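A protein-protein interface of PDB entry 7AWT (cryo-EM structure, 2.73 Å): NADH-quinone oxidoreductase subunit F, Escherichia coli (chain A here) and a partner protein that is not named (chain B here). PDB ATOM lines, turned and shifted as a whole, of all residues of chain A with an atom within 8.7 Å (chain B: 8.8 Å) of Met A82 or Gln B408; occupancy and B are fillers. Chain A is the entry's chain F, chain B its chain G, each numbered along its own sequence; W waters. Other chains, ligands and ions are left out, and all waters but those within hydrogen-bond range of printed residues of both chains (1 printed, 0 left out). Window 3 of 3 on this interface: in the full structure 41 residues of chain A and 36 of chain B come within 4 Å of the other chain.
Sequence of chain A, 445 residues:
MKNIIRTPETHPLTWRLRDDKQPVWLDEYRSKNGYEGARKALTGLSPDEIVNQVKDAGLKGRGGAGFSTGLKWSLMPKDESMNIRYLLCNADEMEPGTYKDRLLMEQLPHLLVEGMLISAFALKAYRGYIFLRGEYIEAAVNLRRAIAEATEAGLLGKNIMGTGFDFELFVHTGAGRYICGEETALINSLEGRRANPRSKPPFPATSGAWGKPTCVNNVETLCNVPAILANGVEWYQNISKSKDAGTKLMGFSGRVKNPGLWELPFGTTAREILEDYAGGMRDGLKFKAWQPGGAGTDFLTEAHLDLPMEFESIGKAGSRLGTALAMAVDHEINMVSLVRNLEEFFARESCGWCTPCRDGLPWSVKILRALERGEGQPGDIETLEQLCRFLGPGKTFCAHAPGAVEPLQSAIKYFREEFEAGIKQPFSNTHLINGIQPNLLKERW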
ATOM      1  N   MET A  76       1.285  17.346 -28.865  1.00  0.00           N
ATOM      2  CA  MET A  76       0.907  18.509 -28.078  1.00  0.00           C
ATOM      3  C   MET A  76       0.963  18.174 -26.590  1.00  0.00           C
ATOM      4  O   MET A  76       0.635  17.051 -26.194  1.00  0.00           O
ATOM      5  CB  MET A  76      -0.499  18.977 -28.452  1.00  0.00           C
ATOM      6  CG  MET A  76      -0.619  19.556 -29.850  1.00  0.00           C
ATOM      7  SD  MET A  76      -0.124  21.282 -29.947  1.00  0.00           S
ATOM      8  CE  MET A  76      -1.548  21.994 -30.768  1.00  0.00           C
ATOM      9  N   PRO A  77       1.372  19.115 -25.742  1.00  0.00           N
ATOM     10  CA  PRO A  77       1.443  18.829 -24.309  1.00  0.00           C
ATOM     11  C   PRO A  77       0.060  18.662 -23.708  1.00  0.00           C
ATOM     12  O   PRO A  77      -0.903  19.322 -24.106  1.00  0.00           O
ATOM     13  CB  PRO A  77       2.151  20.060 -23.738  1.00  0.00           C
ATOM     14  CG  PRO A  77       1.827  21.140 -24.694  1.00  0.00           C
ATOM     15  CD  PRO A  77       1.785  20.495 -26.045  1.00  0.00           C
ATOM     16  N   LYS A  78      -0.030  17.762 -22.735  1.00  0.00           N
ATOM     17  CA  LYS A  78      -1.285  17.435 -22.067  1.00  0.00           C
ATOM     18  C   LYS A  78      -1.252  18.042 -20.668  1.00  0.00           C
ATOM     19  O   LYS A  78      -0.876  17.383 -19.697  1.00  0.00           O
ATOM     20  CB  LYS A  78      -1.501  15.927 -22.020  1.00  0.00           C
ATOM     21  CG  LYS A  78      -1.481  15.262 -23.383  1.00  0.00           C
ATOM     22  CD  LYS A  78      -1.273  13.761 -23.275  1.00  0.00           C
ATOM     23  CE  LYS A  78      -0.985  13.150 -24.637  1.00  0.00           C
ATOM     24  NZ  LYS A  78      -0.849  11.670 -24.569  1.00  0.00           N
ATOM     25  N   ASP A  79      -1.651  19.308 -20.573  1.00  0.00           N
ATOM     26  CA  ASP A  79      -1.821  19.990 -19.300  1.00  0.00           C
ATOM     27  C   ASP A  79      -2.636  21.250 -19.537  1.00  0.00           C
ATOM     28  O   ASP A  79      -2.380  21.986 -20.491  1.00  0.00           O
ATOM     29  CB  ASP A  79      -0.471  20.332 -18.653  1.00  0.00           C
ATOM     30  CG  ASP A  79       0.326  21.340 -19.448  1.00  0.00           C
ATOM     31  OD1 ASP A  79       0.100  22.553 -19.270  1.00  0.00           O
ATOM     32  OD2 ASP A  79       1.183  20.916 -20.249  1.00  0.00           O
ATOM     33  N   GLU A  80      -3.620  21.484 -18.674  1.00  0.00           N
ATOM     34  CA  GLU A  80      -4.512  22.624 -18.828  1.00  0.00           C
ATOM     35  C   GLU A  80      -3.909  23.929 -18.332  1.00  0.00           C
ATOM     36  O   GLU A  80      -4.618  24.939 -18.280  1.00  0.00           O
ATOM     37  CB  GLU A  80      -5.836  22.352 -18.111  1.00  0.00           C
ATOM     38  CG  GLU A  80      -6.906  21.758 -19.016  1.00  0.00           C
ATOM     39  CD  GLU A  80      -6.769  20.258 -19.190  1.00  0.00           C
ATOM     40  OE1 GLU A  80      -7.603  19.664 -19.906  1.00  0.00           O
ATOM     41  OE2 GLU A  80      -5.824  19.674 -18.621  1.00  0.00           O
ATOM     42  N   SER A  81      -2.629  23.937 -17.962  1.00  0.00           N
ATOM     43  CA  SER A  81      -1.939  25.194 -17.709  1.00  0.00           C
ATOM     44  C   SER A  81      -1.621  25.937 -18.996  1.00  0.00           C
ATOM     45  O   SER A  81      -1.357  27.142 -18.952  1.00  0.00           O
ATOM     46  CB  SER A  81      -0.649  24.946 -16.925  1.00  0.00           C
ATOM     47  OG  SER A  81       0.245  24.131 -17.662  1.00  0.00           O
ATOM     48  N   MET A  82      -1.638  25.245 -20.131  1.00  0.00           N
ATOM     49  CA  MET A  82      -1.479  25.845 -21.451  1.00  0.00           C
ATOM     50  C   MET A  82      -2.842  25.777 -22.133  1.00  0.00           C
ATOM     51  O   MET A  82      -3.190  24.773 -22.757  1.00  0.00           O
ATOM     52  CB  MET A  82      -0.415  25.121 -22.265  1.00  0.00           C
ATOM     53  CG  MET A  82       0.965  25.109 -21.642  1.00  0.00           C
ATOM     54  SD  MET A  82       2.122  24.141 -22.626  1.00  0.00           S
ATOM     55  CE  MET A  82       3.596  24.229 -21.619  1.00  0.00           C
ATOM     56  N   ASN A  83      -3.618  26.850 -22.004  1.00  0.00           N
ATOM     57  CA  ASN A  83      -4.957  26.914 -22.569  1.00  0.00           C
ATOM     58  C   ASN A  83      -5.028  27.799 -23.805  1.00  0.00           C
ATOM     59  O   ASN A  83      -6.126  28.132 -24.258  1.00  0.00           O
ATOM     60  CB  ASN A  83      -5.949  27.406 -21.516  1.00  0.00           C
ATOM     61  CG  ASN A  83      -5.420  28.587 -20.732  1.00  0.00           C
ATOM     62  OD1 ASN A  83      -4.324  28.538 -20.180  1.00  0.00           O
ATOM     63  ND2 ASN A  83      -6.201  29.659 -20.682  1.00  0.00           N
ATOM     64  N   ILE A  84      -3.883  28.182 -24.361  1.00  0.00           N
ATOM     65  CA  ILE A  84      -3.815  29.015 -25.556  1.00  0.00           C
ATOM     66  C   ILE A  84      -2.990  28.240 -26.573  1.00  0.00           C
ATOM     67  O   ILE A  84      -1.766  28.136 -26.441  1.00  0.00           O
ATOM     68  CB  ILE A  84      -3.206  30.389 -25.269  1.00  0.00           C
ATOM     69  CG1 ILE A  84      -4.151  31.207 -24.392  1.00  0.00           C
ATOM     70  CG2 ILE A  84      -2.921  31.123 -26.559  1.00  0.00           C
ATOM     71  CD1 ILE A  84      -3.586  32.534 -23.965  1.00  0.00           C
ATOM     72  N   ARG A  85      -3.654  27.677 -27.576  1.00  0.00           N
ATOM     73  CA  ARG A  85      -3.002  26.880 -28.602  1.00  0.00           C
ATOM     74  C   ARG A  85      -3.484  27.332 -29.969  1.00  0.00           C
ATOM     75  O   ARG A  85      -4.605  27.823 -30.116  1.00  0.00           O
ATOM     76  CB  ARG A  85      -3.283  25.390 -28.416  1.00  0.00           C
ATOM     77  CG  ARG A  85      -3.312  24.961 -26.966  1.00  0.00           C
ATOM     78  CD  ARG A  85      -3.159  23.470 -26.815  1.00  0.00           C
ATOM     79  NE  ARG A  85      -3.060  23.095 -25.411  1.00  0.00           N
ATOM     80  CZ  ARG A  85      -2.673  21.900 -24.985  1.00  0.00           C
ATOM     81  NH1 ARG A  85      -2.613  21.647 -23.689  1.00  0.00           N
ATOM     82  NH2 ARG A  85      -2.354  20.956 -25.857  1.00  0.00           N
ATOM     83  N   TYR A  86      -2.631  27.160 -30.972  1.00  0.00           N
ATOM     84  CA  TYR A  86      -2.906  27.648 -32.312  1.00  0.00           C
ATOM     85  C   TYR A  86      -2.841  26.509 -33.317  1.00  0.00           C
ATOM     86  O   TYR A  86      -2.063  25.565 -33.167  1.00  0.00           O
ATOM     87  CB  TYR A  86      -1.917  28.748 -32.710  1.00  0.00           C
ATOM     88  CG  TYR A  86      -2.066  30.004 -31.893  1.00  0.00           C
ATOM     89  CD1 TYR A  86      -3.148  30.847 -32.079  1.00  0.00           C
ATOM     90  CD2 TYR A  86      -1.134  30.340 -30.924  1.00  0.00           C
ATOM     91  CE1 TYR A  86      -3.294  31.989 -31.331  1.00  0.00           C
ATOM     92  CE2 TYR A  86      -1.276  31.484 -30.172  1.00  0.00           C
ATOM     93  CZ  TYR A  86      -2.357  32.303 -30.378  1.00  0.00           C
ATOM     94  OH  TYR A  86      -2.503  33.445 -29.631  1.00  0.00           O
ATOM     95  N   LEU A 123      -7.429  19.598 -31.119  1.00  0.00           N
ATOM     96  CA  LEU A 123      -6.236  20.168 -30.506  1.00  0.00           C
ATOM     97  C   LEU A 123      -6.431  21.177 -29.384  1.00  0.00           C
ATOM     98  O   LEU A 123      -5.473  21.646 -28.813  1.00  0.00           O
ATOM     99  CB  LEU A 123      -5.431  20.866 -31.578  1.00  0.00           C
ATOM    100  CG  LEU A 123      -4.804  20.017 -32.647  1.00  0.00           C
ATOM    101  CD1 LEU A 123      -4.359  20.936 -33.753  1.00  0.00           C
ATOM    102  CD2 LEU A 123      -3.609  19.345 -32.023  1.00  0.00           C
ATOM    103  N   LYS A 124      -7.670  21.516 -29.074  1.00  0.00           N
ATOM    104  CA  LYS A 124      -7.950  22.506 -28.047  1.00  0.00           C
ATOM    105  C   LYS A 124      -7.327  23.851 -28.364  1.00  0.00           C
ATOM    106  O   LYS A 124      -6.811  24.512 -27.475  1.00  0.00           O
ATOM    107  CB  LYS A 124      -7.419  22.058 -26.695  1.00  0.00           C
ATOM    108  CG  LYS A 124      -7.879  20.698 -26.225  1.00  0.00           C
ATOM    109  CD  LYS A 124      -7.452  20.483 -24.789  1.00  0.00           C
ATOM    110  CE  LYS A 124      -7.196  19.017 -24.521  1.00  0.00           C
ATOM    111  NZ  LYS A 124      -6.145  18.473 -25.425  1.00  0.00           N
ATOM    112  N   ALA A 125      -7.393  24.270 -29.619  1.00  0.00           N
ATOM    113  CA  ALA A 125      -6.809  25.533 -30.036  1.00  0.00           C
ATOM    114  C   ALA A 125      -7.904  26.541 -30.207  1.00  0.00           C
ATOM    115  O   ALA A 125      -8.904  26.245 -30.821  1.00  0.00           O
ATOM    116  CB  ALA A 125      -6.080  25.347 -31.340  1.00  0.00           C
ATOM    117  N   PRO A 201      14.744  20.356 -31.856  1.00  0.00           N
ATOM    118  CA  PRO A 201      13.788  20.696 -30.810  1.00  0.00           C
ATOM    119  C   PRO A 201      14.052  22.068 -30.228  1.00  0.00           C
ATOM    120  O   PRO A 201      15.164  22.542 -30.348  1.00  0.00           O
ATOM    121  CB  PRO A 201      14.054  19.635 -29.760  1.00  0.00           C
ATOM    122  CG  PRO A 201      15.494  19.379 -29.893  1.00  0.00           C
ATOM    123  CD  PRO A 201      15.731  19.390 -31.368  1.00  0.00           C
ATOM    124  N   PRO A 202      13.056  22.711 -29.608  1.00  0.00           N
ATOM    125  CA  PRO A 202      11.668  22.348 -29.336  1.00  0.00           C
ATOM    126  C   PRO A 202      10.843  22.344 -30.588  1.00  0.00           C
ATOM    127  O   PRO A 202      11.052  23.181 -31.432  1.00  0.00           O
ATOM    128  CB  PRO A 202      11.177  23.484 -28.444  1.00  0.00           C
ATOM    129  CG  PRO A 202      12.388  24.212 -28.012  1.00  0.00           C
ATOM    130  CD  PRO A 202      13.347  24.063 -29.133  1.00  0.00           C
ATOM    131  N   PHE A 203       9.934  21.397 -30.720  1.00  0.00           N
ATOM    132  CA  PHE A 203       9.089  21.339 -31.893  1.00  0.00           C
ATOM    133  C   PHE A 203       7.985  22.348 -31.773  1.00  0.00           C
ATOM    134  O   PHE A 203       7.665  22.762 -30.683  1.00  0.00           O
ATOM    135  CB  PHE A 203       8.532  19.941 -32.081  1.00  0.00           C
ATOM    136  CG  PHE A 203       9.551  18.969 -32.545  1.00  0.00           C
ATOM    137  CD1 PHE A 203      10.339  18.311 -31.645  1.00  0.00           C
ATOM    138  CD2 PHE A 203       9.751  18.758 -33.877  1.00  0.00           C
ATOM    139  CE1 PHE A 203      11.299  17.437 -32.062  1.00  0.00           C
ATOM    140  CE2 PHE A 203      10.708  17.886 -34.309  1.00  0.00           C
ATOM    141  CZ  PHE A 203      11.483  17.222 -33.399  1.00  0.00           C
ATOM    142  N   ALA A 205       5.107  21.865 -31.815  1.00  0.00           N
ATOM    143  CA  ALA A 205       4.046  21.383 -31.013  1.00  0.00           C
ATOM    144  C   ALA A 205       4.168  21.787 -29.599  1.00  0.00           C
ATOM    145  O   ALA A 205       3.196  21.974 -29.010  1.00  0.00           O
ATOM    146  CB  ALA A 205       3.904  19.913 -31.151  1.00  0.00           C
ATOM    147  N   THR A 206       5.325  21.820 -29.005  1.00  0.00           N
ATOM    148  CA  THR A 206       5.417  22.241 -27.638  1.00  0.00           C
ATOM    149  C   THR A 206       5.553  23.725 -27.485  1.00  0.00           C
ATOM    150  O   THR A 206       5.000  24.273 -26.612  1.00  0.00           O
ATOM    151  CB  THR A 206       6.507  21.498 -26.931  1.00  0.00           C
ATOM    152  OG1 THR A 206       6.635  22.020 -25.632  1.00  0.00           O
ATOM    153  CG2 THR A 206       7.765  21.695 -27.609  1.00  0.00           C
ATOM    154  N   SER A 207       6.324  24.390 -28.318  1.00  0.00           N
ATOM    155  CA  SER A 207       6.422  25.849 -28.295  1.00  0.00           C
ATOM    156  C   SER A 207       6.378  26.223 -29.758  1.00  0.00           C
ATOM    157  O   SER A 207       7.279  25.897 -30.487  1.00  0.00           O
ATOM    158  CB  SER A 207       7.712  26.314 -27.651  1.00  0.00           C
ATOM    159  OG  SER A 207       8.728  26.493 -28.610  1.00  0.00           O
ATOM    160  N   GLY A 208       5.399  26.991 -30.169  1.00  0.00           N
ATOM    161  CA  GLY A 208       5.200  27.269 -31.577  1.00  0.00           C
ATOM    162  C   GLY A 208       4.988  28.722 -31.943  1.00  0.00           C
ATOM    163  O   GLY A 208       5.947  29.492 -32.032  1.00  0.00           O
ATOM    164  N   GLY A 211       5.204  31.281 -28.642  1.00  0.00           N
ATOM    165  CA  GLY A 211       5.571  30.554 -27.451  1.00  0.00           C
ATOM    166  C   GLY A 211       4.524  29.578 -26.977  1.00  0.00           C
ATOM    167  O   GLY A 211       4.777  28.837 -26.021  1.00  0.00           O
ATOM    168  N   LYS A 212       3.362  29.559 -27.610  1.00  0.00           N
ATOM    169  CA  LYS A 212       2.284  28.638 -27.286  1.00  0.00           C
ATOM    170  C   LYS A 212       2.394  27.392 -28.148  1.00  0.00           C
ATOM    171  O   LYS A 212       3.136  27.365 -29.130  1.00  0.00           O
ATOM    172  CB  LYS A 212       0.945  29.337 -27.503  1.00  0.00           C
ATOM    173  CG  LYS A 212       0.908  30.767 -27.012  1.00  0.00           C
ATOM    174  CD  LYS A 212       1.128  30.845 -25.518  1.00  0.00           C
ATOM    175  CE  LYS A 212       0.918  32.256 -25.016  1.00  0.00           C
ATOM    176  NZ  LYS A 212       1.769  33.223 -25.753  1.00  0.00           N
ATOM    177  N   PRO A 213       1.679  26.321 -27.801  1.00  0.00           N
ATOM    178  CA  PRO A 213       1.653  25.152 -28.682  1.00  0.00           C
ATOM    179  C   PRO A 213       1.110  25.514 -30.054  1.00  0.00           C
ATOM    180  O   PRO A 213       0.374  26.487 -30.223  1.00  0.00           O
ATOM    181  CB  PRO A 213       0.723  24.179 -27.954  1.00  0.00           C
ATOM    182  CG  PRO A 213       0.805  24.578 -26.541  1.00  0.00           C
ATOM    183  CD  PRO A 213       0.976  26.060 -26.534  1.00  0.00           C
ATOM    184  N   THR A 214       1.483  24.712 -31.048  1.00  0.00           N
ATOM    185  CA  THR A 214       1.101  24.995 -32.425  1.00  0.00           C
ATOM    186  C   THR A 214       1.325  23.787 -33.320  1.00  0.00           C
ATOM    187  O   THR A 214       2.403  23.189 -33.302  1.00  0.00           O
ATOM    188  CB  THR A 214       1.890  26.189 -32.964  1.00  0.00           C
ATOM    189  OG1 THR A 214       1.359  27.395 -32.409  1.00  0.00           O
ATOM    190  CG2 THR A 214       1.800  26.257 -34.471  1.00  0.00           C
ATOM    191  N   ALA B 401      12.366  34.842 -19.295  1.00  0.00           N
ATOM    192  CA  ALA B 401      12.384  33.972 -20.465  1.00  0.00           C
ATOM    193  C   ALA B 401      13.251  32.748 -20.218  1.00  0.00           C
ATOM    194  O   ALA B 401      12.890  31.632 -20.606  1.00  0.00           O
ATOM    195  CB  ALA B 401      12.872  34.743 -21.687  1.00  0.00           C
ATOM    196  N   ARG B 402      14.390  32.932 -19.548  1.00  0.00           N
ATOM    197  CA  ARG B 402      15.255  31.798 -19.243  1.00  0.00           C
ATOM    198  C   ARG B 402      14.590  30.844 -18.260  1.00  0.00           C
ATOM    199  O   ARG B 402      14.757  29.626 -18.366  1.00  0.00           O
ATOM    200  CB  ARG B 402      16.592  32.288 -18.695  1.00  0.00           C
ATOM    201  CG  ARG B 402      17.399  33.101 -19.683  1.00  0.00           C
ATOM    202  CD  ARG B 402      18.819  33.310 -19.199  1.00  0.00           C
ATOM    203  NE  ARG B 402      19.226  34.705 -19.318  1.00  0.00           N
ATOM    204  CZ  ARG B 402      19.277  35.557 -18.302  1.00  0.00           C
ATOM    205  NH1 ARG B 402      18.950  35.159 -17.082  1.00  0.00           N
ATOM    206  NH2 ARG B 402      19.656  36.808 -18.504  1.00  0.00           N
ATOM    207  N   GLU B 403      13.820  31.371 -17.307  1.00  0.00           N
ATOM    208  CA  GLU B 403      13.093  30.506 -16.385  1.00  0.00           C
ATOM    209  C   GLU B 403      12.005  29.723 -17.111  1.00  0.00           C
ATOM    210  O   GLU B 403      11.847  28.516 -16.895  1.00  0.00           O
ATOM    211  CB  GLU B 403      12.486  31.329 -15.253  1.00  0.00           C
ATOM    212  CG  GLU B 403      13.489  31.845 -14.248  1.00  0.00           C
ATOM    213  CD  GLU B 403      12.834  32.645 -13.144  1.00  0.00           C
ATOM    214  OE1 GLU B 403      11.593  32.770 -13.160  1.00  0.00           O
ATOM    215  OE2 GLU B 403      13.557  33.152 -12.263  1.00  0.00           O
ATOM    216  N   MET B 404      11.235  30.403 -17.964  1.00  0.00           N
ATOM    217  CA  MET B 404      10.212  29.723 -18.751  1.00  0.00           C
ATOM    218  C   MET B 404      10.817  28.658 -19.652  1.00  0.00           C
ATOM    219  O   MET B 404      10.180  27.634 -19.914  1.00  0.00           O
ATOM    220  CB  MET B 404       9.441  30.732 -19.597  1.00  0.00           C
ATOM    221  CG  MET B 404       8.535  31.655 -18.821  1.00  0.00           C
ATOM    222  SD  MET B 404       7.798  32.889 -19.899  1.00  0.00           S
ATOM    223  CE  MET B 404       6.502  33.519 -18.845  1.00  0.00           C
ATOM    224  N   ALA B 405      12.035  28.884 -20.144  1.00  0.00           N
ATOM    225  CA  ALA B 405      12.669  27.902 -21.012  1.00  0.00           C
ATOM    226  C   ALA B 405      13.227  26.730 -20.218  1.00  0.00           C
ATOM    227  O   ALA B 405      13.131  25.580 -20.659  1.00  0.00           O
ATOM    228  CB  ALA B 405      13.774  28.562 -21.831  1.00  0.00           C
ATOM    229  N   ALA B 406      13.813  26.992 -19.052  1.00  0.00           N
ATOM    230  CA  ALA B 406      14.323  25.909 -18.225  1.00  0.00           C
ATOM    231  C   ALA B 406      13.205  25.079 -17.615  1.00  0.00           C
ATOM    232  O   ALA B 406      13.427  23.909 -17.292  1.00  0.00           O
ATOM    233  CB  ALA B 406      15.219  26.464 -17.120  1.00  0.00           C
ATOM    234  N   ALA B 407      12.015  25.653 -17.445  1.00  0.00           N
ATOM    235  CA  ALA B 407      10.881  24.870 -16.975  1.00  0.00           C
ATOM    236  C   ALA B 407      10.352  23.927 -18.047  1.00  0.00           C
ATOM    237  O   ALA B 407       9.640  22.974 -17.717  1.00  0.00           O
ATOM    238  CB  ALA B 407       9.761  25.793 -16.497  1.00  0.00           C
ATOM    239  N   GLN B 408      10.677  24.173 -19.314  1.00  0.00           N
ATOM    240  CA  GLN B 408      10.269  23.317 -20.417  1.00  0.00           C
ATOM    241  C   GLN B 408      11.413  22.454 -20.930  1.00  0.00           C
ATOM    242  O   GLN B 408      11.332  21.932 -22.048  1.00  0.00           O
ATOM    243  CB  GLN B 408       9.693  24.156 -21.556  1.00  0.00           C
ATOM    244  CG  GLN B 408       8.486  24.980 -21.163  1.00  0.00           C
ATOM    245  CD  GLN B 408       7.725  25.494 -22.362  1.00  0.00           C
ATOM    246  OE1 GLN B 408       7.922  25.026 -23.481  1.00  0.00           O
ATOM    247  NE2 GLN B 408       6.850  26.465 -22.136  1.00  0.00           N
ATOM    248  N   LYS B 409      12.477  22.308 -20.142  1.00  0.00           N
ATOM    249  CA  LYS B 409      13.626  21.472 -20.493  1.00  0.00           C
ATOM    250  C   LYS B 409      14.289  21.945 -21.783  1.00  0.00           C
ATOM    251  O   LYS B 409      14.667  21.144 -22.639  1.00  0.00           O
ATOM    252  CB  LYS B 409      13.228  19.999 -20.594  1.00  0.00           C
ATOM    253  CG  LYS B 409      12.686  19.423 -19.300  1.00  0.00           C
ATOM    254  CD  LYS B 409      13.748  19.425 -18.220  1.00  0.00           C
ATOM    255  CE  LYS B 409      13.240  18.785 -16.943  1.00  0.00           C
ATOM    256  NZ  LYS B 409      14.270  18.804 -15.868  1.00  0.00           N
ATOM    257  N   VAL B 410      14.432  23.258 -21.925  1.00  0.00           N
ATOM    258  CA  VAL B 410      15.172  23.857 -23.028  1.00  0.00           C
ATOM    259  C   VAL B 410      16.553  24.235 -22.515  1.00  0.00           C
ATOM    260  O   VAL B 410      16.680  24.835 -21.441  1.00  0.00           O
ATOM    261  CB  VAL B 410      14.436  25.081 -23.600  1.00  0.00           C
ATOM    262  CG1 VAL B 410      15.289  25.767 -24.644  1.00  0.00           C
ATOM    263  CG2 VAL B 410      13.112  24.667 -24.201  1.00  0.00           C
ATOM    264  N   ALA B 411      17.584  23.876 -23.272  1.00  0.00           N
ATOM    265  CA  ALA B 411      18.946  24.163 -22.853  1.00  0.00           C
ATOM    266  C   ALA B 411      19.185  25.667 -22.800  1.00  0.00           C
ATOM    267  O   ALA B 411      18.573  26.440 -23.538  1.00  0.00           O
ATOM    268  CB  ALA B 411      19.938  23.505 -23.804  1.00  0.00           C
ATOM    269  N   ALA B 417      15.208  29.516 -28.948  1.00  0.00           N
ATOM    270  CA  ALA B 417      14.063  28.930 -28.264  1.00  0.00           C
ATOM    271  C   ALA B 417      13.758  29.647 -26.958  1.00  0.00           C
ATOM    272  O   ALA B 417      12.588  29.809 -26.603  1.00  0.00           O
ATOM    273  CB  ALA B 417      14.314  27.451 -28.003  1.00  0.00           C
ATOM    274  N   ASN B 420      11.992  32.820 -28.000  1.00  0.00           N
ATOM    275  CA  ASN B 420      10.694  32.505 -28.525  1.00  0.00           C
ATOM    276  C   ASN B 420       9.730  32.131 -27.422  1.00  0.00           C
ATOM    277  O   ASN B 420       8.575  32.420 -27.530  1.00  0.00           O
ATOM    278  CB  ASN B 420      10.790  31.387 -29.523  1.00  0.00           C
ATOM    279  CG  ASN B 420       9.473  30.760 -29.780  1.00  0.00           C
ATOM    280  OD1 ASN B 420       8.478  31.438 -29.879  1.00  0.00           O
ATOM    281  ND2 ASN B 420       9.458  29.456 -29.885  1.00  0.00           N
ATOM    282  N   ILE B 421      10.188  31.449 -26.384  1.00  0.00           N
ATOM    283  CA  ILE B 421       9.311  31.048 -25.290  1.00  0.00           C
ATOM    284  C   ILE B 421       8.943  32.250 -24.432  1.00  0.00           C
ATOM    285  O   ILE B 421       7.822  32.346 -23.924  1.00  0.00           O
ATOM    286  CB  ILE B 421       9.972  29.932 -24.465  1.00  0.00           C
ATOM    287  CG1 ILE B 421       9.938  28.616 -25.239  1.00  0.00           C
ATOM    288  CG2 ILE B 421       9.283  29.762 -23.134  1.00  0.00           C
ATOM    289  CD1 ILE B 421      10.579  27.470 -24.511  1.00  0.00           C
ATOM    290  N   GLY B 422       9.868  33.191 -24.271  1.00  0.00           N
ATOM    291  CA  GLY B 422       9.605  34.395 -23.512  1.00  0.00           C
ATOM    292  C   GLY B 422       8.512  35.254 -24.110  1.00  0.00           C
ATOM    293  O   GLY B 422       7.477  35.468 -23.477  1.00  0.00           O
HETATM  294  O   HOH W   1       5.146  31.178 -23.696  1.00  0.00           O
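The side-chain hydroxyl of Ser A207 lies within hydrogen-bond range of the side-chain amide nitrogen of Asn B420 (3.3 Å).
The backbone carbonyl oxygen (O) of Met A82 sits at hydrogen-bond distance from the guanidinium group (NE) of Arg A85 (3.1 Å).
The backbone carbonyl oxygen (O) of Ala B405 sits at hydrogen-bond distance from the backbone NH (N) of Val B410, 2.9 Å away.
OD1 of Asp A79 sits at hydrogen-bond distance from N of Met A82 (3.3 Å).
CE of Met A82 touches NE2 of Gln B408 (3.98 Å).
Val B410 touches Pro A202.
Pro A202 touches Ala B417.
OE1 of Gln B408 touches OG1 of Thr A206, at 3.9 Å.
O of Gly A208 touches OD1 of Asn B420, at 3.9 Å.
N of Gly A211 touches OD1 of Asn B420, 3.5 Å away.
Of the printed residues of chain B, Met A82 touches Gln B408.
Printed residues of chain A within 4 Å of Gln B408: Met A82 and Thr A206.
Ser A81 touches none of the printed residues of chain B.
Of the printed residues of chain A, Asn B420 touches Ser A207 (3.3 Å), Gly A208 (3.9 Å) and Gly A211 (3.5 Å).
Of the printed residues of chain B, Gly A208 touches Asn B420.
Printed residues of chain A within 4 Å of Ala B417: Pro A202 (3.7 Å).
Of the printed residues of chain B, Gly A211 touches Asn B420.
Glu B403 touches none of the printed residues of chain A.
Glu A80 touches none of the printed residues of chain B.
Of the 25 printed residues of chain A, 6 touch a printed residue of chain B.
Printed residues of chain A that touch a printed residue of chain B: Met A82, Pro A202, Thr A206, Ser A207, Gly A208 and Gly A211.
Printed residues of chain B that touch a printed residue of chain A: Gln B408, Val B410, Ala B417 and Asn B420.
Hydrophobic or aromatic side chains of chain B that line the printed part of chain A: Val B410 and Ala B417.
Water W1 lies within hydrogen-bond range of O of Ile B421 and O of Gly A211.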
